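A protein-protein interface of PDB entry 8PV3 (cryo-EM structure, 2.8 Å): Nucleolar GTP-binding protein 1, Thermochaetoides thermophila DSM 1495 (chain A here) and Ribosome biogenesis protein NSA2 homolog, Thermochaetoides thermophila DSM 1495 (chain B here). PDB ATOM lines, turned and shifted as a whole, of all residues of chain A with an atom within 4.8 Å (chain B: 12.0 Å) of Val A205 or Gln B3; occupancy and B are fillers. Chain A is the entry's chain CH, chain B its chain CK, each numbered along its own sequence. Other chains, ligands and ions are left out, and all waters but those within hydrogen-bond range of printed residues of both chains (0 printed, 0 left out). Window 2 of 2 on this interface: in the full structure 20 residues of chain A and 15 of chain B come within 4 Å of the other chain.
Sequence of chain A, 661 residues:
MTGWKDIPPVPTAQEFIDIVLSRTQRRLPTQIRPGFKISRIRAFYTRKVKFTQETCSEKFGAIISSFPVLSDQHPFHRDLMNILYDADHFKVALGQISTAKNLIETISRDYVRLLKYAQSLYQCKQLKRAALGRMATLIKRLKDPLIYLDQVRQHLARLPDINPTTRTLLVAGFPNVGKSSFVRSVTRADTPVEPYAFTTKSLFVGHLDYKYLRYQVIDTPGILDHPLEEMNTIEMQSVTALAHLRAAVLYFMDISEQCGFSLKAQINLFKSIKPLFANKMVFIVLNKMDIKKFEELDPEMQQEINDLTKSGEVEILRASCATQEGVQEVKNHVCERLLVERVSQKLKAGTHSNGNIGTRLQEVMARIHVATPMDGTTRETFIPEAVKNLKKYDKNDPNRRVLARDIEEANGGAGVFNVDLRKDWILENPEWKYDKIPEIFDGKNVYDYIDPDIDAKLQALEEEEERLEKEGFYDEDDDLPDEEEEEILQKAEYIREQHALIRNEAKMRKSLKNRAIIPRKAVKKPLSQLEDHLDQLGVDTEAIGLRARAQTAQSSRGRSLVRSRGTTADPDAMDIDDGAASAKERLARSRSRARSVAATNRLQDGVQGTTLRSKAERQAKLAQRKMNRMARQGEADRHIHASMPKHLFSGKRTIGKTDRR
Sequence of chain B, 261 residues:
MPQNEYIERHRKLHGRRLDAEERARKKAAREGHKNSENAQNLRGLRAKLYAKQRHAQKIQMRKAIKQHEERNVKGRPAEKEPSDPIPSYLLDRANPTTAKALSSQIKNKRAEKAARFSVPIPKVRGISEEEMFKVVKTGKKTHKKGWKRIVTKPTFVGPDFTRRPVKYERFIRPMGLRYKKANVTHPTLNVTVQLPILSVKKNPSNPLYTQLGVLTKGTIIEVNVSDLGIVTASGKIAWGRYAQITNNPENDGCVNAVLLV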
ATOM      1  N   ARG A 158     -16.781  21.118   5.721  1.00  0.00           N
ATOM      2  CA  ARG A 158     -17.900  21.519   4.875  1.00  0.00           C
ATOM      3  C   ARG A 158     -17.479  22.148   3.548  1.00  0.00           C
ATOM      4  O   ARG A 158     -18.355  22.529   2.767  1.00  0.00           O
ATOM      5  CB  ARG A 158     -18.812  22.484   5.630  1.00  0.00           C
ATOM      6  CG  ARG A 158     -19.369  21.910   6.910  1.00  0.00           C
ATOM      7  CD  ARG A 158     -20.525  22.736   7.420  1.00  0.00           C
ATOM      8  NE  ARG A 158     -20.177  24.142   7.562  1.00  0.00           N
ATOM      9  CZ  ARG A 158     -19.647  24.671   8.654  1.00  0.00           C
ATOM     10  NH1 ARG A 158     -19.354  23.929   9.708  1.00  0.00           N
ATOM     11  NH2 ARG A 158     -19.404  25.976   8.689  1.00  0.00           N
ATOM     12  N   PRO A 160     -16.364  22.523  -0.346  1.00  0.00           N
ATOM     13  CA  PRO A 160     -16.542  21.701  -1.550  1.00  0.00           C
ATOM     14  C   PRO A 160     -15.229  21.109  -2.033  1.00  0.00           C
ATOM     15  O   PRO A 160     -14.147  21.625  -1.742  1.00  0.00           O
ATOM     16  CB  PRO A 160     -17.109  22.687  -2.576  1.00  0.00           C
ATOM     17  CG  PRO A 160     -16.737  24.027  -2.073  1.00  0.00           C
ATOM     18  CD  PRO A 160     -16.731  23.928  -0.582  1.00  0.00           C
ATOM     19  N   ASP A 161     -15.334  20.017  -2.787  1.00  0.00           N
ATOM     20  CA  ASP A 161     -14.168  19.350  -3.364  1.00  0.00           C
ATOM     21  C   ASP A 161     -14.024  19.790  -4.813  1.00  0.00           C
ATOM     22  O   ASP A 161     -14.768  19.343  -5.688  1.00  0.00           O
ATOM     23  CB  ASP A 161     -14.310  17.837  -3.263  1.00  0.00           C
ATOM     24  CG  ASP A 161     -12.994  17.112  -3.467  1.00  0.00           C
ATOM     25  OD1 ASP A 161     -11.954  17.789  -3.599  1.00  0.00           O
ATOM     26  OD2 ASP A 161     -12.999  15.865  -3.498  1.00  0.00           O
ATOM     27  N   ILE A 162     -13.055  20.659  -5.076  1.00  0.00           N
ATOM     28  CA  ILE A 162     -12.812  21.197  -6.408  1.00  0.00           C
ATOM     29  C   ILE A 162     -11.484  20.642  -6.902  1.00  0.00           C
ATOM     30  O   ILE A 162     -10.437  20.863  -6.284  1.00  0.00           O
ATOM     31  CB  ILE A 162     -12.806  22.729  -6.409  1.00  0.00           C
ATOM     32  CG1 ILE A 162     -14.207  23.261  -6.108  1.00  0.00           C
ATOM     33  CG2 ILE A 162     -12.292  23.258  -7.735  1.00  0.00           C
ATOM     34  CD1 ILE A 162     -14.275  24.758  -5.966  1.00  0.00           C
ATOM     35  N   ALA A 189     -26.300  20.879  -8.410  1.00  0.00           N
ATOM     36  CA  ALA A 189     -25.864  21.560  -7.198  1.00  0.00           C
ATOM     37  C   ALA A 189     -26.986  22.412  -6.623  1.00  0.00           C
ATOM     38  O   ALA A 189     -27.756  23.031  -7.361  1.00  0.00           O
ATOM     39  CB  ALA A 189     -24.645  22.430  -7.491  1.00  0.00           C
ATOM     40  N   LEU A 203     -17.853  29.420  -2.624  1.00  0.00           N
ATOM     41  CA  LEU A 203     -17.802  28.676  -3.875  1.00  0.00           C
ATOM     42  C   LEU A 203     -18.725  27.465  -3.822  1.00  0.00           C
ATOM     43  O   LEU A 203     -18.732  26.710  -2.847  1.00  0.00           O
ATOM     44  CB  LEU A 203     -16.370  28.232  -4.167  1.00  0.00           C
ATOM     45  CG  LEU A 203     -15.330  29.341  -4.326  1.00  0.00           C
ATOM     46  CD1 LEU A 203     -13.934  28.757  -4.401  1.00  0.00           C
ATOM     47  CD2 LEU A 203     -15.626  30.171  -5.556  1.00  0.00           C
ATOM     48  N   PHE A 204     -19.509  27.284  -4.881  1.00  0.00           N
ATOM     49  CA  PHE A 204     -20.349  26.110  -5.054  1.00  0.00           C
ATOM     50  C   PHE A 204     -19.871  25.368  -6.289  1.00  0.00           C
ATOM     51  O   PHE A 204     -19.294  25.976  -7.193  1.00  0.00           O
ATOM     52  CB  PHE A 204     -21.825  26.485  -5.219  1.00  0.00           C
ATOM     53  CG  PHE A 204     -22.540  26.756  -3.928  1.00  0.00           C
ATOM     54  CD1 PHE A 204     -22.456  27.995  -3.318  1.00  0.00           C
ATOM     55  CD2 PHE A 204     -23.316  25.774  -3.334  1.00  0.00           C
ATOM     56  CE1 PHE A 204     -23.122  28.246  -2.133  1.00  0.00           C
ATOM     57  CE2 PHE A 204     -23.984  26.021  -2.151  1.00  0.00           C
ATOM     58  CZ  PHE A 204     -23.890  27.259  -1.552  1.00  0.00           C
ATOM     59  N   VAL A 205     -20.106  24.063  -6.337  1.00  0.00           N
ATOM     60  CA  VAL A 205     -19.694  23.254  -7.476  1.00  0.00           C
ATOM     61  C   VAL A 205     -20.796  22.259  -7.822  1.00  0.00           C
ATOM     62  O   VAL A 205     -21.414  21.657  -6.939  1.00  0.00           O
ATOM     63  CB  VAL A 205     -18.339  22.557  -7.204  1.00  0.00           C
ATOM     64  CG1 VAL A 205     -18.390  21.722  -5.951  1.00  0.00           C
ATOM     65  CG2 VAL A 205     -17.898  21.720  -8.391  1.00  0.00           C
ATOM     66  N   GLY A 206     -21.081  22.144  -9.123  1.00  0.00           N
ATOM     67  CA  GLY A 206     -21.934  21.099  -9.634  1.00  0.00           C
ATOM     68  C   GLY A 206     -21.205  20.336 -10.725  1.00  0.00           C
ATOM     69  O   GLY A 206     -20.071  20.654 -11.071  1.00  0.00           O
ATOM     70  N   HIS A 207     -21.872  19.319 -11.257  1.00  0.00           N
ATOM     71  CA  HIS A 207     -21.265  18.470 -12.270  1.00  0.00           C
ATOM     72  C   HIS A 207     -22.265  18.192 -13.381  1.00  0.00           C
ATOM     73  O   HIS A 207     -23.474  18.119 -13.150  1.00  0.00           O
ATOM     74  CB  HIS A 207     -20.768  17.150 -11.672  1.00  0.00           C
ATOM     75  CG  HIS A 207     -19.665  17.315 -10.673  1.00  0.00           C
ATOM     76  ND1 HIS A 207     -19.888  17.721  -9.376  1.00  0.00           N
ATOM     77  CD2 HIS A 207     -18.329  17.119 -10.780  1.00  0.00           C
ATOM     78  CE1 HIS A 207     -18.739  17.779  -8.729  1.00  0.00           C
ATOM     79  NE2 HIS A 207     -17.778  17.415  -9.556  1.00  0.00           N
ATOM     80  N   GLN A 216     -17.001  19.811 -14.372  1.00  0.00           N
ATOM     81  CA  GLN A 216     -17.417  20.451 -13.133  1.00  0.00           C
ATOM     82  C   GLN A 216     -17.632  21.940 -13.377  1.00  0.00           C
ATOM     83  O   GLN A 216     -16.887  22.570 -14.131  1.00  0.00           O
ATOM     84  CB  GLN A 216     -16.409  20.199 -12.007  1.00  0.00           C
ATOM     85  CG  GLN A 216     -15.073  20.886 -12.133  1.00  0.00           C
ATOM     86  CD  GLN A 216     -14.183  20.641 -10.936  1.00  0.00           C
ATOM     87  OE1 GLN A 216     -14.528  19.874 -10.040  1.00  0.00           O
ATOM     88  NE2 GLN A 216     -13.032  21.299 -10.910  1.00  0.00           N
ATOM     89  N   VAL A 217     -18.685  22.484 -12.774  1.00  0.00           N
ATOM     90  CA  VAL A 217     -19.103  23.867 -12.957  1.00  0.00           C
ATOM     91  C   VAL A 217     -19.018  24.558 -11.606  1.00  0.00           C
ATOM     92  O   VAL A 217     -19.589  24.077 -10.624  1.00  0.00           O
ATOM     93  CB  VAL A 217     -20.534  23.954 -13.520  1.00  0.00           C
ATOM     94  CG1 VAL A 217     -20.898  25.389 -13.838  1.00  0.00           C
ATOM     95  CG2 VAL A 217     -20.682  23.071 -14.747  1.00  0.00           C
ATOM     96  N   ILE A 218     -18.317  25.684 -11.553  1.00  0.00           N
ATOM     97  CA  ILE A 218     -18.038  26.370 -10.298  1.00  0.00           C
ATOM     98  C   ILE A 218     -18.767  27.705 -10.289  1.00  0.00           C
ATOM     99  O   ILE A 218     -18.487  28.589 -11.111  1.00  0.00           O
ATOM    100  CB  ILE A 218     -16.532  26.558 -10.081  1.00  0.00           C
ATOM    101  CG1 ILE A 218     -15.829  25.205 -10.130  1.00  0.00           C
ATOM    102  CG2 ILE A 218     -16.270  27.238  -8.753  1.00  0.00           C
ATOM    103  CD1 ILE A 218     -14.339  25.301 -10.124  1.00  0.00           C
ATOM    104  N   PRO B   2     -22.644  17.190   0.105  1.00  0.00           N
ATOM    105  CA  PRO B   2     -23.135  18.523   0.446  1.00  0.00           C
ATOM    106  C   PRO B   2     -21.973  19.479   0.642  1.00  0.00           C
ATOM    107  O   PRO B   2     -20.841  19.036   0.805  1.00  0.00           O
ATOM    108  CB  PRO B   2     -23.894  18.283   1.742  1.00  0.00           C
ATOM    109  CG  PRO B   2     -23.174  17.162   2.373  1.00  0.00           C
ATOM    110  CD  PRO B   2     -22.644  16.298   1.273  1.00  0.00           C
ATOM    111  N   GLN B   3     -22.245  20.778   0.612  1.00  0.00           N
ATOM    112  CA  GLN B   3     -21.201  21.785   0.680  1.00  0.00           C
ATOM    113  C   GLN B   3     -21.720  23.006   1.423  1.00  0.00           C
ATOM    114  O   GLN B   3     -22.920  23.294   1.406  1.00  0.00           O
ATOM    115  CB  GLN B   3     -20.734  22.182  -0.719  1.00  0.00           C
ATOM    116  CG  GLN B   3     -21.880  22.448  -1.675  1.00  0.00           C
ATOM    117  CD  GLN B   3     -21.445  22.481  -3.118  1.00  0.00           C
ATOM    118  OE1 GLN B   3     -20.281  22.718  -3.418  1.00  0.00           O
ATOM    119  NE2 GLN B   3     -22.385  22.255  -4.025  1.00  0.00           N
ATOM    120  N   ASN B   4     -20.797  23.704   2.076  1.00  0.00           N
ATOM    121  CA  ASN B   4     -21.036  24.955   2.821  1.00  0.00           C
ATOM    122  C   ASN B   4     -22.026  24.654   3.951  1.00  0.00           C
ATOM    123  O   ASN B   4     -21.900  23.618   4.619  1.00  0.00           O
ATOM    124  CB  ASN B   4     -21.441  26.048   1.857  1.00  0.00           C
ATOM    125  CG  ASN B   4     -20.494  26.151   0.679  1.00  0.00           C
ATOM    126  OD1 ASN B   4     -19.281  26.230   0.853  1.00  0.00           O
ATOM    127  ND2 ASN B   4     -21.041  26.142  -0.524  1.00  0.00           N
ATOM    128  N   GLU B   5     -23.010  25.515   4.200  1.00  0.00           N
ATOM    129  CA  GLU B   5     -23.871  25.381   5.377  1.00  0.00           C
ATOM    130  C   GLU B   5     -25.128  24.583   5.026  1.00  0.00           C
ATOM    131  O   GLU B   5     -26.252  25.091   4.982  1.00  0.00           O
ATOM    132  CB  GLU B   5     -24.207  26.755   5.938  1.00  0.00           C
ATOM    133  CG  GLU B   5     -23.002  27.472   6.514  1.00  0.00           C
ATOM    134  CD  GLU B   5     -23.297  28.908   6.888  1.00  0.00           C
ATOM    135  OE1 GLU B   5     -24.391  29.402   6.548  1.00  0.00           O
ATOM    136  OE2 GLU B   5     -22.431  29.543   7.524  1.00  0.00           O
ATOM    137  N   TYR B   6     -24.915  23.284   4.803  1.00  0.00           N
ATOM    138  CA  TYR B   6     -25.982  22.453   4.255  1.00  0.00           C
ATOM    139  C   TYR B   6     -27.024  22.092   5.308  1.00  0.00           C
ATOM    140  O   TYR B   6     -28.204  21.933   4.983  1.00  0.00           O
ATOM    141  CB  TYR B   6     -25.405  21.196   3.606  1.00  0.00           C
ATOM    142  CG  TYR B   6     -24.414  20.409   4.431  1.00  0.00           C
ATOM    143  CD1 TYR B   6     -24.842  19.400   5.282  1.00  0.00           C
ATOM    144  CD2 TYR B   6     -23.051  20.631   4.313  1.00  0.00           C
ATOM    145  CE1 TYR B   6     -23.945  18.662   6.019  1.00  0.00           C
ATOM    146  CE2 TYR B   6     -22.144  19.895   5.044  1.00  0.00           C
ATOM    147  CZ  TYR B   6     -22.599  18.911   5.895  1.00  0.00           C
ATOM    148  OH  TYR B   6     -21.702  18.175   6.630  1.00  0.00           O
ATOM    149  N   ILE B   7     -26.619  21.962   6.574  1.00  0.00           N
ATOM    150  CA  ILE B   7     -27.606  21.675   7.613  1.00  0.00           C
ATOM    151  C   ILE B   7     -28.488  22.894   7.859  1.00  0.00           C
ATOM    152  O   ILE B   7     -29.700  22.759   8.058  1.00  0.00           O
ATOM    153  CB  ILE B   7     -26.913  21.180   8.899  1.00  0.00           C
ATOM    154  CG1 ILE B   7     -26.393  19.756   8.702  1.00  0.00           C
ATOM    155  CG2 ILE B   7     -27.853  21.188  10.097  1.00  0.00           C
ATOM    156  CD1 ILE B   7     -27.468  18.739   8.422  1.00  0.00           C
ATOM    157  N   GLU B   8     -27.921  24.100   7.797  1.00  0.00           N
ATOM    158  CA  GLU B   8     -28.743  25.303   7.892  1.00  0.00           C
ATOM    159  C   GLU B   8     -29.638  25.471   6.670  1.00  0.00           C
ATOM    160  O   GLU B   8     -30.758  25.981   6.781  1.00  0.00           O
ATOM    161  CB  GLU B   8     -27.861  26.532   8.081  1.00  0.00           C
ATOM    162  CG  GLU B   8     -27.216  26.621   9.447  1.00  0.00           C
ATOM    163  CD  GLU B   8     -26.239  27.770   9.548  1.00  0.00           C
ATOM    164  OE1 GLU B   8     -26.299  28.679   8.694  1.00  0.00           O
ATOM    165  OE2 GLU B   8     -25.396  27.755  10.468  1.00  0.00           O
ATOM    166  N   ARG B   9     -29.171  25.053   5.490  1.00  0.00           N
ATOM    167  CA  ARG B   9     -30.042  25.122   4.320  1.00  0.00           C
ATOM    168  C   ARG B   9     -31.188  24.117   4.418  1.00  0.00           C
ATOM    169  O   ARG B   9     -32.326  24.423   4.040  1.00  0.00           O
ATOM    170  CB  ARG B   9     -29.228  24.910   3.044  1.00  0.00           C
ATOM    171  CG  ARG B   9     -30.073  24.889   1.788  1.00  0.00           C
ATOM    172  CD  ARG B   9     -29.464  25.698   0.661  1.00  0.00           C
ATOM    173  NE  ARG B   9     -30.341  25.709  -0.502  1.00  0.00           N
ATOM    174  CZ  ARG B   9     -31.392  26.506  -0.640  1.00  0.00           C
ATOM    175  NH1 ARG B   9     -31.727  27.378   0.296  1.00  0.00           N
ATOM    176  NH2 ARG B   9     -32.129  26.424  -1.744  1.00  0.00           N
ATOM    177  N   HIS B  10     -30.909  22.922   4.941  1.00  0.00           N
ATOM    178  CA  HIS B  10     -31.963  21.947   5.200  1.00  0.00           C
ATOM    179  C   HIS B  10     -32.923  22.454   6.263  1.00  0.00           C
ATOM    180  O   HIS B  10     -34.126  22.169   6.216  1.00  0.00           O
ATOM    181  CB  HIS B  10     -31.344  20.620   5.630  1.00  0.00           C
ATOM    182  CG  HIS B  10     -32.339  19.518   5.809  1.00  0.00           C
ATOM    183  ND1 HIS B  10     -32.744  18.710   4.773  1.00  0.00           N
ATOM    184  CD2 HIS B  10     -32.994  19.076   6.906  1.00  0.00           C
ATOM    185  CE1 HIS B  10     -33.617  17.827   5.221  1.00  0.00           C
ATOM    186  NE2 HIS B  10     -33.786  18.026   6.513  1.00  0.00           N
ATOM    187  N   ARG B  11     -32.393  23.192   7.239  1.00  0.00           N
ATOM    188  CA  ARG B  11     -33.212  23.844   8.253  1.00  0.00           C
ATOM    189  C   ARG B  11     -34.160  24.862   7.631  1.00  0.00           C
ATOM    190  O   ARG B  11     -35.330  24.956   8.024  1.00  0.00           O
ATOM    191  CB  ARG B  11     -32.293  24.531   9.252  1.00  0.00           C
ATOM    192  CG  ARG B  11     -32.906  25.005  10.543  1.00  0.00           C
ATOM    193  CD  ARG B  11     -31.798  25.224  11.565  1.00  0.00           C
ATOM    194  NE  ARG B  11     -31.194  23.979  12.026  1.00  0.00           N
ATOM    195  CZ  ARG B  11     -29.937  23.857  12.430  1.00  0.00           C
ATOM    196  NH1 ARG B  11     -29.116  24.895  12.459  1.00  0.00           N
ATOM    197  NH2 ARG B  11     -29.494  22.665  12.813  1.00  0.00           N
ATOM    198  N   LEU B  13     -35.193  24.833   4.436  1.00  0.00           N
ATOM    199  CA  LEU B  13     -36.121  24.202   3.502  1.00  0.00           C
ATOM    200  C   LEU B  13     -37.177  23.352   4.199  1.00  0.00           C
ATOM    201  O   LEU B  13     -38.347  23.381   3.800  1.00  0.00           O
ATOM    202  CB  LEU B  13     -35.348  23.344   2.502  1.00  0.00           C
ATOM    203  CG  LEU B  13     -34.514  24.118   1.480  1.00  0.00           C
ATOM    204  CD1 LEU B  13     -33.638  23.176   0.678  1.00  0.00           C
ATOM    205  CD2 LEU B  13     -35.388  24.944   0.560  1.00  0.00           C
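Val A205 touches just one residue of chain B: Gln B3 (3.1 Å). Of chain A, only Arg A158 (3.6 Å), Pro A160 (3.3 Å), Phe A204 (3.7 Å) and Val A205 (3.1 Å) come within 4 Å of Gln B3. No residue of chain B comes within 4 Å of Ile A162. No residue of chain B comes within 4 Å of Ala A189. No residue of chain B comes within 4 Å of His A207. No residue of chain B comes within 4 Å of Gln A216. Val A217 touches none of the printed residues of chain B. No residue of chain B comes within 4 Å of Ile A218. Printed residues of chain A within 4 Å of Tyr B6: Arg A158. Printed residues of chain B within 4 Å of Leu A203: Asn B4 (3.3 Å). Of the printed residues of chain B, Arg A158 touches Gln B3 (3.6 Å), Asn B4 (2.8 Å) and Tyr B6 (3.9 Å). Of the printed residues of chain A, Asn B4 touches Arg A158, Pro A160, Leu A203 and Phe A204. His B10 touches none of the printed residues of chain A. Ile B7 touches none of the printed residues of chain A.
The backbone carbonyl oxygen (O) of Val A205 lies within hydrogen-bond range of the side-chain amide nitrogen (NE2) of Gln B3, at 3.1 Å. O of Arg A158 sits at hydrogen-bond distance from N of Asn B4. ND2 of Asn B4 lies within hydrogen-bond range of O of Leu A203, at 3.3 Å.
Of the 13 printed residues of chain A, 5 touch a printed residue of chain B. Hydrophobic or aromatic side chains of chain A within 4 Å of the printed part of chain B: Pro A160, Phe A204 and Val A205.
Gln B3 touches Arg A158. Tyr B6 touches Arg A158. Pro A160 touches Gln B3. Pro A160 touches Asn B4. NE2 of Gln B3 touches CD2 of Phe A204 (3.7 Å). Phe A204 touches Asn B4.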
